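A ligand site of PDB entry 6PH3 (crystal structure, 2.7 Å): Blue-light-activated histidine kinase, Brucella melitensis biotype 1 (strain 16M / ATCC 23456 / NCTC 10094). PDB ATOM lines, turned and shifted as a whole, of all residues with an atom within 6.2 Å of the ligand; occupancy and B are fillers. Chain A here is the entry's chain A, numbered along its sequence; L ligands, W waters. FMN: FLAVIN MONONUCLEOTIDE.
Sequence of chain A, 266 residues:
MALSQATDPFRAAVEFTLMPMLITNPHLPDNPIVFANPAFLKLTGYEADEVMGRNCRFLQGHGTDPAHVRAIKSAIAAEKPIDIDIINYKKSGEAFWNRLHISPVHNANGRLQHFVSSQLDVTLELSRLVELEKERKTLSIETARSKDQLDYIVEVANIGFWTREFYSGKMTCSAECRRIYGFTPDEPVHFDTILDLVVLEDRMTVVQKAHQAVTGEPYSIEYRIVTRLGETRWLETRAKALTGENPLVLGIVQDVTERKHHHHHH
Water W1 lies within hydrogen-bond range of the backbone carbonyl oxygen of Asn 31 (2.7 Å), the side-chain amide nitrogen of Asn 55 (2.8 Å), the side-chain sulfur of Cys 56 (3.1 Å) and an oxygen (O2') of the ligand (3.1 Å).
NH1 of Arg 57 is in salt-bridge range of O2P of the ligand, at 2.7 Å.
OD1 of Asn 88 lies within hydrogen-bond range of N3 of the ligand (2.8 Å).
An oxygen (O4') of the ligand lies within hydrogen-bond range of the side-chain amide nitrogen of Gln 60, at 2.8 Å.
An oxygen (O2') of the ligand is in hydrogen-bond range of the side-chain amide oxygen of Asn 55, at 2.9 Å.
The side-chain amide nitrogen (ND2) of Asn 98 is in hydrogen-bond range of an oxygen (O4) of the ligand (3.0 Å).
The side-chain amide nitrogen (NE2) of Gln 119 lies close to an oxygen (O4) of the ligand (3.2 Å).
The side-chain amino group (NZ) of Lys 73 is in salt-bridge range of an oxygen (O2P) of the ligand.
The backbone NH of Cys 56 sits at hydrogen-bond distance from an oxygen (O2') of the ligand (3.4 Å).
The side-chain amide oxygen (OD1) of Asn 88 sits at hydrogen-bond distance from the side-chain amide nitrogen (ND2) of Asn 98 (2.8 Å).
The backbone carbonyl oxygen (O) of Leu 59 sits close to the side-chain amide nitrogen (ND2) of Asn 88 (3.4 Å).
The side-chain amide nitrogen of Asn 55 lies within hydrogen-bond range of the backbone carbonyl oxygen of Asp 30.
OD1 of Asn 98 sits close to N of Leu 100.
N of Asn 98 lies within hydrogen-bond range of O of Ile 86 (2.8 Å).
The side-chain amide nitrogen (NE2) of Gln 119 lies within hydrogen-bond range of the side-chain hydroxyl (OG) of Ser 117 (2.7 Å).
The backbone carbonyl oxygen (O) of Phe 115 is in hydrogen-bond range of the backbone NH (N) of Thr 24 (3.1 Å).
The backbone carbonyl oxygen (O) of Val 116 lies within hydrogen-bond range of the backbone NH (N) of Ser 103, 2.9 Å away.
Residues that only touch the ligand: Thr 24 (3.8 Å), Asn 31 (3.2 Å), Leu 59 (3.3 Å), Val 69 (3.6 Å), Ile 72 (3.5 Å), Ile 76 (3.4 Å), Ile 86 (3.9 Å), Leu 100 (3.6 Å), Ile 102 (3.6 Å), Phe 115 (3.7 Å), Val 116 (3.9 Å) and Ser 117 (3.5 Å).
Hydrophobic or aromatic side chains that line the ligand: Leu 59, Val 69, Ile 72, Ile 76, Ile 86, Leu 100, Ile 102 and Phe 115.
Within 4 Å of the ligand: Thr 24, Asn 31, Asn 55, Cys 56, Arg 57, Leu 59, Gln 60, Val 69, Ile 72, Lys 73, Ile 76, Ile 86, Asn 88, Asn 98, Leu 100, Ile 102, Phe 115, Val 116, Ser 117 and Gln 119.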
ATOM      1  N   LEU A  22       9.643  22.973 -12.950  1.00  0.00           N
ATOM      2  CA  LEU A  22      10.444  23.967 -12.221  1.00  0.00           C
ATOM      3  C   LEU A  22      10.996  23.437 -10.909  1.00  0.00           C
ATOM      4  O   LEU A  22      10.331  22.676 -10.211  1.00  0.00           O
ATOM      5  CB  LEU A  22       9.622  25.227 -11.926  1.00  0.00           C
ATOM      6  CG  LEU A  22       9.086  26.038 -13.099  1.00  0.00           C
ATOM      7  CD1 LEU A  22       8.439  27.301 -12.587  1.00  0.00           C
ATOM      8  CD2 LEU A  22      10.193  26.391 -14.089  1.00  0.00           C
ATOM      9  N   ILE A  23      12.187  23.886 -10.558  1.00  0.00           N
ATOM     10  CA  ILE A  23      12.813  23.587  -9.273  1.00  0.00           C
ATOM     11  C   ILE A  23      13.216  24.938  -8.667  1.00  0.00           C
ATOM     12  O   ILE A  23      13.930  25.696  -9.313  1.00  0.00           O
ATOM     13  CB  ILE A  23      14.006  22.594  -9.355  1.00  0.00           C
ATOM     14  CG1 ILE A  23      13.617  21.260 -10.081  1.00  0.00           C
ATOM     15  CG2 ILE A  23      14.584  22.320  -7.953  1.00  0.00           C
ATOM     16  CD1 ILE A  23      14.785  20.323 -10.449  1.00  0.00           C
ATOM     17  N   THR A  24      12.727  25.259  -7.468  1.00  0.00           N
ATOM     18  CA  THR A  24      13.103  26.510  -6.778  1.00  0.00           C
ATOM     19  C   THR A  24      13.910  26.191  -5.503  1.00  0.00           C
ATOM     20  O   THR A  24      13.984  25.012  -5.097  1.00  0.00           O
ATOM     21  CB  THR A  24      11.887  27.343  -6.466  1.00  0.00           C
ATOM     22  OG1 THR A  24      11.216  26.735  -5.367  1.00  0.00           O
ATOM     23  CG2 THR A  24      10.955  27.576  -7.691  1.00  0.00           C
ATOM     24  N   ASP A  30      13.203  34.970  -1.766  1.00  0.00           N
ATOM     25  CA  ASP A  30      11.977  34.958  -2.547  1.00  0.00           C
ATOM     26  C   ASP A  30      11.682  33.620  -3.266  1.00  0.00           C
ATOM     27  O   ASP A  30      10.835  33.589  -4.158  1.00  0.00           O
ATOM     28  CB  ASP A  30      11.959  36.150  -3.536  1.00  0.00           C
ATOM     29  CG  ASP A  30      10.588  36.588  -3.971  1.00  0.00           C
ATOM     30  OD1 ASP A  30       9.609  36.249  -3.273  1.00  0.00           O
ATOM     31  OD2 ASP A  30      10.497  37.237  -5.044  1.00  0.00           O
ATOM     32  N   ASN A  31      12.329  32.509  -2.828  1.00  0.00           N
ATOM     33  CA  ASN A  31      12.155  31.149  -3.390  1.00  0.00           C
ATOM     34  C   ASN A  31      12.262  31.196  -4.937  1.00  0.00           C
ATOM     35  O   ASN A  31      11.269  31.002  -5.636  1.00  0.00           O
ATOM     36  CB  ASN A  31      10.831  30.530  -2.906  1.00  0.00           C
ATOM     37  CG  ASN A  31      10.658  29.070  -3.187  1.00  0.00           C
ATOM     38  OD1 ASN A  31      11.601  28.297  -3.209  1.00  0.00           O
ATOM     39  ND2 ASN A  31       9.446  28.630  -3.307  1.00  0.00           N
ATOM     40  N   PHE A  40       9.207  23.628 -20.297  1.00  0.00           N
ATOM     41  CA  PHE A  40       8.654  24.819 -19.627  1.00  0.00           C
ATOM     42  C   PHE A  40       8.900  26.078 -20.450  1.00  0.00           C
ATOM     43  O   PHE A  40       7.988  26.901 -20.603  1.00  0.00           O
ATOM     44  CB  PHE A  40       9.230  24.964 -18.227  1.00  0.00           C
ATOM     45  CG  PHE A  40       8.695  26.171 -17.498  1.00  0.00           C
ATOM     46  CD1 PHE A  40       7.527  26.076 -16.737  1.00  0.00           C
ATOM     47  CD2 PHE A  40       9.369  27.384 -17.535  1.00  0.00           C
ATOM     48  CE1 PHE A  40       7.045  27.190 -16.049  1.00  0.00           C
ATOM     49  CE2 PHE A  40       8.862  28.512 -16.863  1.00  0.00           C
ATOM     50  CZ  PHE A  40       7.716  28.397 -16.116  1.00  0.00           C
ATOM     51  N   ASN A  55      10.937  34.434  -8.717  1.00  0.00           N
ATOM     52  CA  ASN A  55       9.848  33.663  -8.085  1.00  0.00           C
ATOM     53  C   ASN A  55       8.914  33.375  -9.270  1.00  0.00           C
ATOM     54  O   ASN A  55       8.984  34.128 -10.241  1.00  0.00           O
ATOM     55  CB  ASN A  55       9.149  34.452  -6.974  1.00  0.00           C
ATOM     56  CG  ASN A  55       8.069  33.690  -6.184  1.00  0.00           C
ATOM     57  OD1 ASN A  55       6.887  33.784  -6.481  1.00  0.00           O
ATOM     58  ND2 ASN A  55       8.437  32.887  -5.187  1.00  0.00           N
ATOM     59  N   CYS A  56       8.114  32.270  -9.227  1.00  0.00           N
ATOM     60  CA  CYS A  56       7.241  31.807 -10.333  1.00  0.00           C
ATOM     61  C   CYS A  56       6.026  32.653 -10.547  1.00  0.00           C
ATOM     62  O   CYS A  56       5.301  32.433 -11.510  1.00  0.00           O
ATOM     63  CB  CYS A  56       6.867  30.339 -10.155  1.00  0.00           C
ATOM     64  SG  CYS A  56       8.217  29.335  -9.487  1.00  0.00           S
ATOM     65  N   ARG A  57       5.816  33.620  -9.675  1.00  0.00           N
ATOM     66  CA  ARG A  57       4.743  34.617  -9.672  1.00  0.00           C
ATOM     67  C   ARG A  57       4.486  35.252 -11.010  1.00  0.00           C
ATOM     68  O   ARG A  57       3.350  35.642 -11.260  1.00  0.00           O
ATOM     69  CB  ARG A  57       5.130  35.756  -8.729  1.00  0.00           C
ATOM     70  CG  ARG A  57       4.286  35.843  -7.509  1.00  0.00           C
ATOM     71  CD  ARG A  57       4.524  37.165  -6.798  1.00  0.00           C
ATOM     72  NE  ARG A  57       5.915  37.341  -6.406  1.00  0.00           N
ATOM     73  CZ  ARG A  57       6.487  36.842  -5.307  1.00  0.00           C
ATOM     74  NH1 ARG A  57       5.786  36.084  -4.475  1.00  0.00           N
ATOM     75  NH2 ARG A  57       7.752  37.088  -5.045  1.00  0.00           N
ATOM     76  N   LEU A  59       4.086  34.266 -13.806  1.00  0.00           N
ATOM     77  CA  LEU A  59       3.123  33.529 -14.629  1.00  0.00           C
ATOM     78  C   LEU A  59       1.700  34.034 -14.399  1.00  0.00           C
ATOM     79  O   LEU A  59       0.856  33.887 -15.265  1.00  0.00           O
ATOM     80  CB  LEU A  59       3.241  32.004 -14.412  1.00  0.00           C
ATOM     81  CG  LEU A  59       4.534  31.400 -14.889  1.00  0.00           C
ATOM     82  CD1 LEU A  59       4.795  30.108 -14.217  1.00  0.00           C
ATOM     83  CD2 LEU A  59       4.556  31.285 -16.392  1.00  0.00           C
ATOM     84  N   GLN A  60       1.447  34.652 -13.259  1.00  0.00           N
ATOM     85  CA  GLN A  60       0.153  35.214 -12.883  1.00  0.00           C
ATOM     86  C   GLN A  60      -0.113  36.572 -13.580  1.00  0.00           C
ATOM     87  O   GLN A  60       0.830  37.338 -13.862  1.00  0.00           O
ATOM     88  CB  GLN A  60       0.072  35.396 -11.364  1.00  0.00           C
ATOM     89  CG  GLN A  60       0.139  34.082 -10.599  1.00  0.00           C
ATOM     90  CD  GLN A  60       0.733  34.187  -9.225  1.00  0.00           C
ATOM     91  OE1 GLN A  60       0.740  35.241  -8.544  1.00  0.00           O
ATOM     92  NE2 GLN A  60       1.192  33.051  -8.733  1.00  0.00           N
ATOM     93  N   THR A  64      -5.958  35.896 -13.108  1.00  0.00           N
ATOM     94  CA  THR A  64      -5.583  34.967 -12.040  1.00  0.00           C
ATOM     95  C   THR A  64      -6.467  35.235 -10.811  1.00  0.00           C
ATOM     96  O   THR A  64      -6.540  36.374 -10.340  1.00  0.00           O
ATOM     97  CB  THR A  64      -4.078  35.073 -11.704  1.00  0.00           C
ATOM     98  OG1 THR A  64      -3.307  34.982 -12.892  1.00  0.00           O
ATOM     99  CG2 THR A  64      -3.618  34.008 -10.756  1.00  0.00           C
ATOM    100  N   VAL A  69      -3.987  31.923  -5.633  1.00  0.00           N
ATOM    101  CA  VAL A  69      -2.681  32.419  -5.201  1.00  0.00           C
ATOM    102  C   VAL A  69      -2.507  32.208  -3.703  1.00  0.00           C
ATOM    103  O   VAL A  69      -1.428  31.822  -3.257  1.00  0.00           O
ATOM    104  CB  VAL A  69      -2.454  33.894  -5.618  1.00  0.00           C
ATOM    105  CG1 VAL A  69      -1.029  34.335  -5.333  1.00  0.00           C
ATOM    106  CG2 VAL A  69      -2.788  34.104  -7.085  1.00  0.00           C
ATOM    107  N   ARG A  70      -3.609  32.449  -2.938  1.00  0.00           N
ATOM    108  CA  ARG A  70      -3.744  32.321  -1.473  1.00  0.00           C
ATOM    109  C   ARG A  70      -3.522  30.863  -1.058  1.00  0.00           C
ATOM    110  O   ARG A  70      -2.847  30.610  -0.058  1.00  0.00           O
ATOM    111  CB  ARG A  70      -5.150  32.792  -1.066  1.00  0.00           C
ATOM    112  CG  ARG A  70      -5.340  33.347   0.359  1.00  0.00           C
ATOM    113  CD  ARG A  70      -6.780  33.838   0.576  1.00  0.00           C
ATOM    114  NE  ARG A  70      -7.154  34.914  -0.370  1.00  0.00           N
ATOM    115  CZ  ARG A  70      -8.302  34.968  -1.052  1.00  0.00           C
ATOM    116  NH1 ARG A  70      -9.233  34.020  -0.894  1.00  0.00           N
ATOM    117  NH2 ARG A  70      -8.542  35.976  -1.879  1.00  0.00           N
ATOM    118  N   ILE A  72      -1.880  28.453  -2.773  1.00  0.00           N
ATOM    119  CA  ILE A  72      -0.466  28.160  -3.085  1.00  0.00           C
ATOM    120  C   ILE A  72       0.428  28.708  -1.972  1.00  0.00           C
ATOM    121  O   ILE A  72       1.220  27.955  -1.416  1.00  0.00           O
ATOM    122  CB  ILE A  72      -0.055  28.758  -4.456  1.00  0.00           C
ATOM    123  CG1 ILE A  72      -0.861  28.154  -5.624  1.00  0.00           C
ATOM    124  CG2 ILE A  72       1.445  28.623  -4.661  1.00  0.00           C
ATOM    125  CD1 ILE A  72      -0.699  28.852  -6.938  1.00  0.00           C
ATOM    126  N   LYS A  73       0.299  30.035  -1.672  1.00  0.00           N
ATOM    127  CA  LYS A  73       1.041  30.738  -0.602  1.00  0.00           C
ATOM    128  C   LYS A  73       0.961  29.949   0.719  1.00  0.00           C
ATOM    129  O   LYS A  73       1.992  29.676   1.335  1.00  0.00           O
ATOM    130  CB  LYS A  73       0.518  32.175  -0.439  1.00  0.00           C
ATOM    131  CG  LYS A  73       1.212  32.996   0.635  1.00  0.00           C
ATOM    132  CD  LYS A  73       1.271  34.494   0.378  1.00  0.00           C
ATOM    133  CE  LYS A  73       2.339  35.126   1.240  1.00  0.00           C
ATOM    134  NZ  LYS A  73       3.606  34.298   1.248  1.00  0.00           N
ATOM    135  N   ILE A  76       2.723  26.306   0.478  1.00  0.00           N
ATOM    136  CA  ILE A  76       4.171  26.487   0.470  1.00  0.00           C
ATOM    137  C   ILE A  76       4.655  26.790   1.899  1.00  0.00           C
ATOM    138  O   ILE A  76       5.631  26.179   2.359  1.00  0.00           O
ATOM    139  CB  ILE A  76       4.610  27.518  -0.605  1.00  0.00           C
ATOM    140  CG1 ILE A  76       4.376  26.947  -2.027  1.00  0.00           C
ATOM    141  CG2 ILE A  76       6.074  27.946  -0.407  1.00  0.00           C
ATOM    142  CD1 ILE A  76       4.469  27.868  -3.140  1.00  0.00           C
ATOM    143  N   ILE A  86      -5.099  26.898 -12.191  1.00  0.00           N
ATOM    144  CA  ILE A  86      -4.943  28.352 -12.108  1.00  0.00           C
ATOM    145  C   ILE A  86      -4.695  28.960 -13.492  1.00  0.00           C
ATOM    146  O   ILE A  86      -4.067  28.297 -14.333  1.00  0.00           O
ATOM    147  CB  ILE A  86      -3.831  28.678 -11.043  1.00  0.00           C
ATOM    148  CG1 ILE A  86      -3.780  30.177 -10.680  1.00  0.00           C
ATOM    149  CG2 ILE A  86      -2.435  28.131 -11.474  1.00  0.00           C
ATOM    150  CD1 ILE A  86      -2.816  30.583  -9.531  1.00  0.00           C
ATOM    151  N   ILE A  87      -5.227  30.188 -13.745  1.00  0.00           N
ATOM    152  CA  ILE A  87      -5.008  30.919 -14.987  1.00  0.00           C
ATOM    153  C   ILE A  87      -3.601  31.561 -14.923  1.00  0.00           C
ATOM    154  O   ILE A  87      -3.275  32.330 -13.994  1.00  0.00           O
ATOM    155  CB  ILE A  87      -6.112  31.946 -15.295  1.00  0.00           C
ATOM    156  CG1 ILE A  87      -7.390  31.247 -15.754  1.00  0.00           C
ATOM    157  CG2 ILE A  87      -5.629  32.983 -16.345  1.00  0.00           C
ATOM    158  CD1 ILE A  87      -8.690  32.008 -15.380  1.00  0.00           C
ATOM    159  N   ASN A  88      -2.781  31.222 -15.915  1.00  0.00           N
ATOM    160  CA  ASN A  88      -1.436  31.727 -16.026  1.00  0.00           C
ATOM    161  C   ASN A  88      -1.274  32.326 -17.429  1.00  0.00           C
ATOM    162  O   ASN A  88      -2.093  32.059 -18.299  1.00  0.00           O
ATOM    163  CB  ASN A  88      -0.414  30.606 -15.744  1.00  0.00           C
ATOM    164  CG  ASN A  88       0.127  30.458 -14.339  1.00  0.00           C
ATOM    165  OD1 ASN A  88       0.983  29.584 -14.109  1.00  0.00           O
ATOM    166  ND2 ASN A  88      -0.277  31.313 -13.391  1.00  0.00           N
ATOM    167  N   ASN A  98      -3.415  26.367 -16.207  1.00  0.00           N
ATOM    168  CA  ASN A  98      -2.275  25.611 -15.720  1.00  0.00           C
ATOM    169  C   ASN A  98      -2.708  24.651 -14.634  1.00  0.00           C
ATOM    170  O   ASN A  98      -3.067  25.070 -13.541  1.00  0.00           O
ATOM    171  CB  ASN A  98      -1.183  26.575 -15.202  1.00  0.00           C
ATOM    172  CG  ASN A  98       0.086  25.953 -14.650  1.00  0.00           C
ATOM    173  OD1 ASN A  98       0.267  24.739 -14.645  1.00  0.00           O
ATOM    174  ND2 ASN A  98       0.987  26.784 -14.146  1.00  0.00           N
ATOM    175  N   LEU A 100      -1.419  22.951 -12.198  1.00  0.00           N
ATOM    176  CA  LEU A 100      -0.222  23.104 -11.424  1.00  0.00           C
ATOM    177  C   LEU A 100      -0.161  22.107 -10.268  1.00  0.00           C
ATOM    178  O   LEU A 100      -1.174  21.753  -9.659  1.00  0.00           O
ATOM    179  CB  LEU A 100      -0.180  24.565 -10.930  1.00  0.00           C
ATOM    180  CG  LEU A 100       0.913  25.012  -9.973  1.00  0.00           C
ATOM    181  CD1 LEU A 100       2.324  24.817 -10.549  1.00  0.00           C
ATOM    182  CD2 LEU A 100       0.665  26.441  -9.493  1.00  0.00           C
ATOM    183  N   HIS A 101       1.045  21.607 -10.032  1.00  0.00           N
ATOM    184  CA  HIS A 101       1.378  20.778  -8.905  1.00  0.00           C
ATOM    185  C   HIS A 101       2.701  21.317  -8.376  1.00  0.00           C
ATOM    186  O   HIS A 101       3.615  21.568  -9.157  1.00  0.00           O
ATOM    187  CB  HIS A 101       1.498  19.284  -9.247  1.00  0.00           C
ATOM    188  CG  HIS A 101       1.968  18.484  -8.069  1.00  0.00           C
ATOM    189  ND1 HIS A 101       1.070  17.953  -7.147  1.00  0.00           N
ATOM    190  CD2 HIS A 101       3.226  18.240  -7.626  1.00  0.00           C
ATOM    191  CE1 HIS A 101       1.802  17.387  -6.201  1.00  0.00           C
ATOM    192  NE2 HIS A 101       3.113  17.546  -6.443  1.00  0.00           N
ATOM    193  N   ILE A 102       2.761  21.534  -7.048  1.00  0.00           N
ATOM    194  CA  ILE A 102       3.953  21.953  -6.311  1.00  0.00           C
ATOM    195  C   ILE A 102       4.149  20.954  -5.171  1.00  0.00           C
ATOM    196  O   ILE A 102       3.191  20.623  -4.466  1.00  0.00           O
ATOM    197  CB  ILE A 102       3.872  23.406  -5.786  1.00  0.00           C
ATOM    198  CG1 ILE A 102       3.582  24.394  -6.935  1.00  0.00           C
ATOM    199  CG2 ILE A 102       5.172  23.785  -5.044  1.00  0.00           C
ATOM    200  CD1 ILE A 102       2.967  25.629  -6.500  1.00  0.00           C
ATOM    201  N   SER A 103       5.373  20.446  -4.993  1.00  0.00           N
ATOM    202  CA  SER A 103       5.680  19.479  -3.935  1.00  0.00           C
ATOM    203  C   SER A 103       6.964  19.876  -3.239  1.00  0.00           C
ATOM    204  O   SER A 103       7.976  20.170  -3.899  1.00  0.00           O
ATOM    205  CB  SER A 103       5.835  18.061  -4.508  1.00  0.00           C
ATOM    206  OG  SER A 103       5.011  17.080  -3.888  1.00  0.00           O
ATOM    207  N   PHE A 115      11.735  22.893  -3.751  1.00  0.00           N
ATOM    208  CA  PHE A 115      10.350  22.762  -4.168  1.00  0.00           C
ATOM    209  C   PHE A 115      10.394  22.339  -5.626  1.00  0.00           C
ATOM    210  O   PHE A 115      11.247  22.806  -6.385  1.00  0.00           O
ATOM    211  CB  PHE A 115       9.620  24.066  -4.031  1.00  0.00           C
ATOM    212  CG  PHE A 115       8.949  24.248  -2.690  1.00  0.00           C
ATOM    213  CD1 PHE A 115       7.744  23.607  -2.402  1.00  0.00           C
ATOM    214  CD2 PHE A 115       9.481  25.116  -1.749  1.00  0.00           C
ATOM    215  CE1 PHE A 115       7.121  23.793  -1.176  1.00  0.00           C
ATOM    216  CE2 PHE A 115       8.840  25.315  -0.516  1.00  0.00           C
ATOM    217  CZ  PHE A 115       7.665  24.654  -0.235  1.00  0.00           C
ATOM    218  N   VAL A 116       9.518  21.429  -6.014  1.00  0.00           N
ATOM    219  CA  VAL A 116       9.445  20.932  -7.399  1.00  0.00           C
ATOM    220  C   VAL A 116       8.026  21.152  -7.962  1.00  0.00           C
ATOM    221  O   VAL A 116       7.056  21.128  -7.198  1.00  0.00           O
ATOM    222  CB  VAL A 116       9.948  19.473  -7.569  1.00  0.00           C
ATOM    223  CG1 VAL A 116      11.454  19.373  -7.308  1.00  0.00           C
ATOM    224  CG2 VAL A 116       9.160  18.489  -6.694  1.00  0.00           C
ATOM    225  N   SER A 117       7.905  21.378  -9.261  1.00  0.00           N
ATOM    226  CA  SER A 117       6.595  21.578  -9.887  1.00  0.00           C
ATOM    227  C   SER A 117       6.454  20.908 -11.269  1.00  0.00           C
ATOM    228  O   SER A 117       7.452  20.524 -11.879  1.00  0.00           O
ATOM    229  CB  SER A 117       6.285  23.053 -10.013  1.00  0.00           C
ATOM    230  OG  SER A 117       7.038  23.618 -11.073  1.00  0.00           O
ATOM    231  N   SER A 118       5.185  20.770 -11.725  1.00  0.00           N
ATOM    232  CA  SER A 118       4.737  20.288 -13.022  1.00  0.00           C
ATOM    233  C   SER A 118       3.697  21.289 -13.418  1.00  0.00           C
ATOM    234  O   SER A 118       2.819  21.634 -12.618  1.00  0.00           O
ATOM    235  CB  SER A 118       4.051  18.926 -12.904  1.00  0.00           C
ATOM    236  OG  SER A 118       4.730  18.052 -12.029  1.00  0.00           O
ATOM    237  N   GLN A 119       3.806  21.809 -14.649  1.00  0.00           N
ATOM    238  CA  GLN A 119       2.830  22.772 -15.168  1.00  0.00           C
ATOM    239  C   GLN A 119       2.229  22.226 -16.444  1.00  0.00           C
ATOM    240  O   GLN A 119       2.885  22.182 -17.473  1.00  0.00           O
ATOM    241  CB  GLN A 119       3.456  24.144 -15.356  1.00  0.00           C
ATOM    242  CG  GLN A 119       3.816  24.807 -14.052  1.00  0.00           C
ATOM    243  CD  GLN A 119       5.240  24.621 -13.648  1.00  0.00           C
ATOM    244  OE1 GLN A 119       5.958  23.780 -14.178  1.00  0.00           O
ATOM    245  NE2 GLN A 119       5.665  25.360 -12.650  1.00  0.00           N
HETATM  246  N1  FMN L   1       2.489  30.107  -9.420  1.00  0.00           N
HETATM  247  C2  FMN L   1       1.788  30.139 -10.594  1.00  0.00           C
HETATM  248  O2  FMN L   1       0.857  30.928 -10.773  1.00  0.00           O
HETATM  249  N3  FMN L   1       2.109  29.251 -11.614  1.00  0.00           N
HETATM  250  C4  FMN L   1       3.126  28.314 -11.590  1.00  0.00           C
HETATM  251  O4  FMN L   1       3.354  27.613 -12.580  1.00  0.00           O
HETATM  252  C4A FMN L   1       3.866  28.278 -10.335  1.00  0.00           C
HETATM  253  N5  FMN L   1       4.826  27.393 -10.197  1.00  0.00           N
HETATM  254  C5A FMN L   1       5.478  27.314  -8.976  1.00  0.00           C
HETATM  255  C6  FMN L   1       6.437  26.319  -8.789  1.00  0.00           C
HETATM  256  C7  FMN L   1       7.085  26.140  -7.565  1.00  0.00           C
HETATM  257  C7M FMN L   1       8.092  25.043  -7.414  1.00  0.00           C
HETATM  258  C8  FMN L   1       6.771  27.009  -6.487  1.00  0.00           C
HETATM  259  C8M FMN L   1       7.445  26.857  -5.144  1.00  0.00           C
HETATM  260  C9  FMN L   1       5.825  28.011  -6.673  1.00  0.00           C
HETATM  261  C9A FMN L   1       5.166  28.169  -7.900  1.00  0.00           C
HETATM  262  N10 FMN L   1       4.123  29.126  -8.091  1.00  0.00           N
HETATM  263  C10 FMN L   1       3.470  29.218  -9.294  1.00  0.00           C
HETATM  264  C1' FMN L   1       3.663  29.957  -6.967  1.00  0.00           C
HETATM  265  C2' FMN L   1       4.319  31.325  -6.824  1.00  0.00           C
HETATM  266  O2' FMN L   1       5.740  31.218  -6.970  1.00  0.00           O
HETATM  267  C3' FMN L   1       3.997  31.937  -5.455  1.00  0.00           C
HETATM  268  O3' FMN L   1       4.384  31.032  -4.419  1.00  0.00           O
HETATM  269  C4' FMN L   1       2.545  32.376  -5.306  1.00  0.00           C
HETATM  270  O4' FMN L   1       2.309  33.455  -6.220  1.00  0.00           O
HETATM  271  C5' FMN L   1       2.108  32.725  -3.890  1.00  0.00           C
HETATM  272  O5' FMN L   1       3.036  33.632  -3.269  1.00  0.00           O
HETATM  273  P   FMN L   1       2.841  35.243  -3.260  1.00  0.00           P
HETATM  274  O1P FMN L   1       1.492  35.678  -2.745  1.00  0.00           O
HETATM  275  O2P FMN L   1       3.978  35.793  -2.427  1.00  0.00           O
HETATM  276  O3P FMN L   1       3.009  35.687  -4.676  1.00  0.00           O
HETATM  277  O   HOH W   1       8.800  30.560  -6.663  1.00  0.00           O
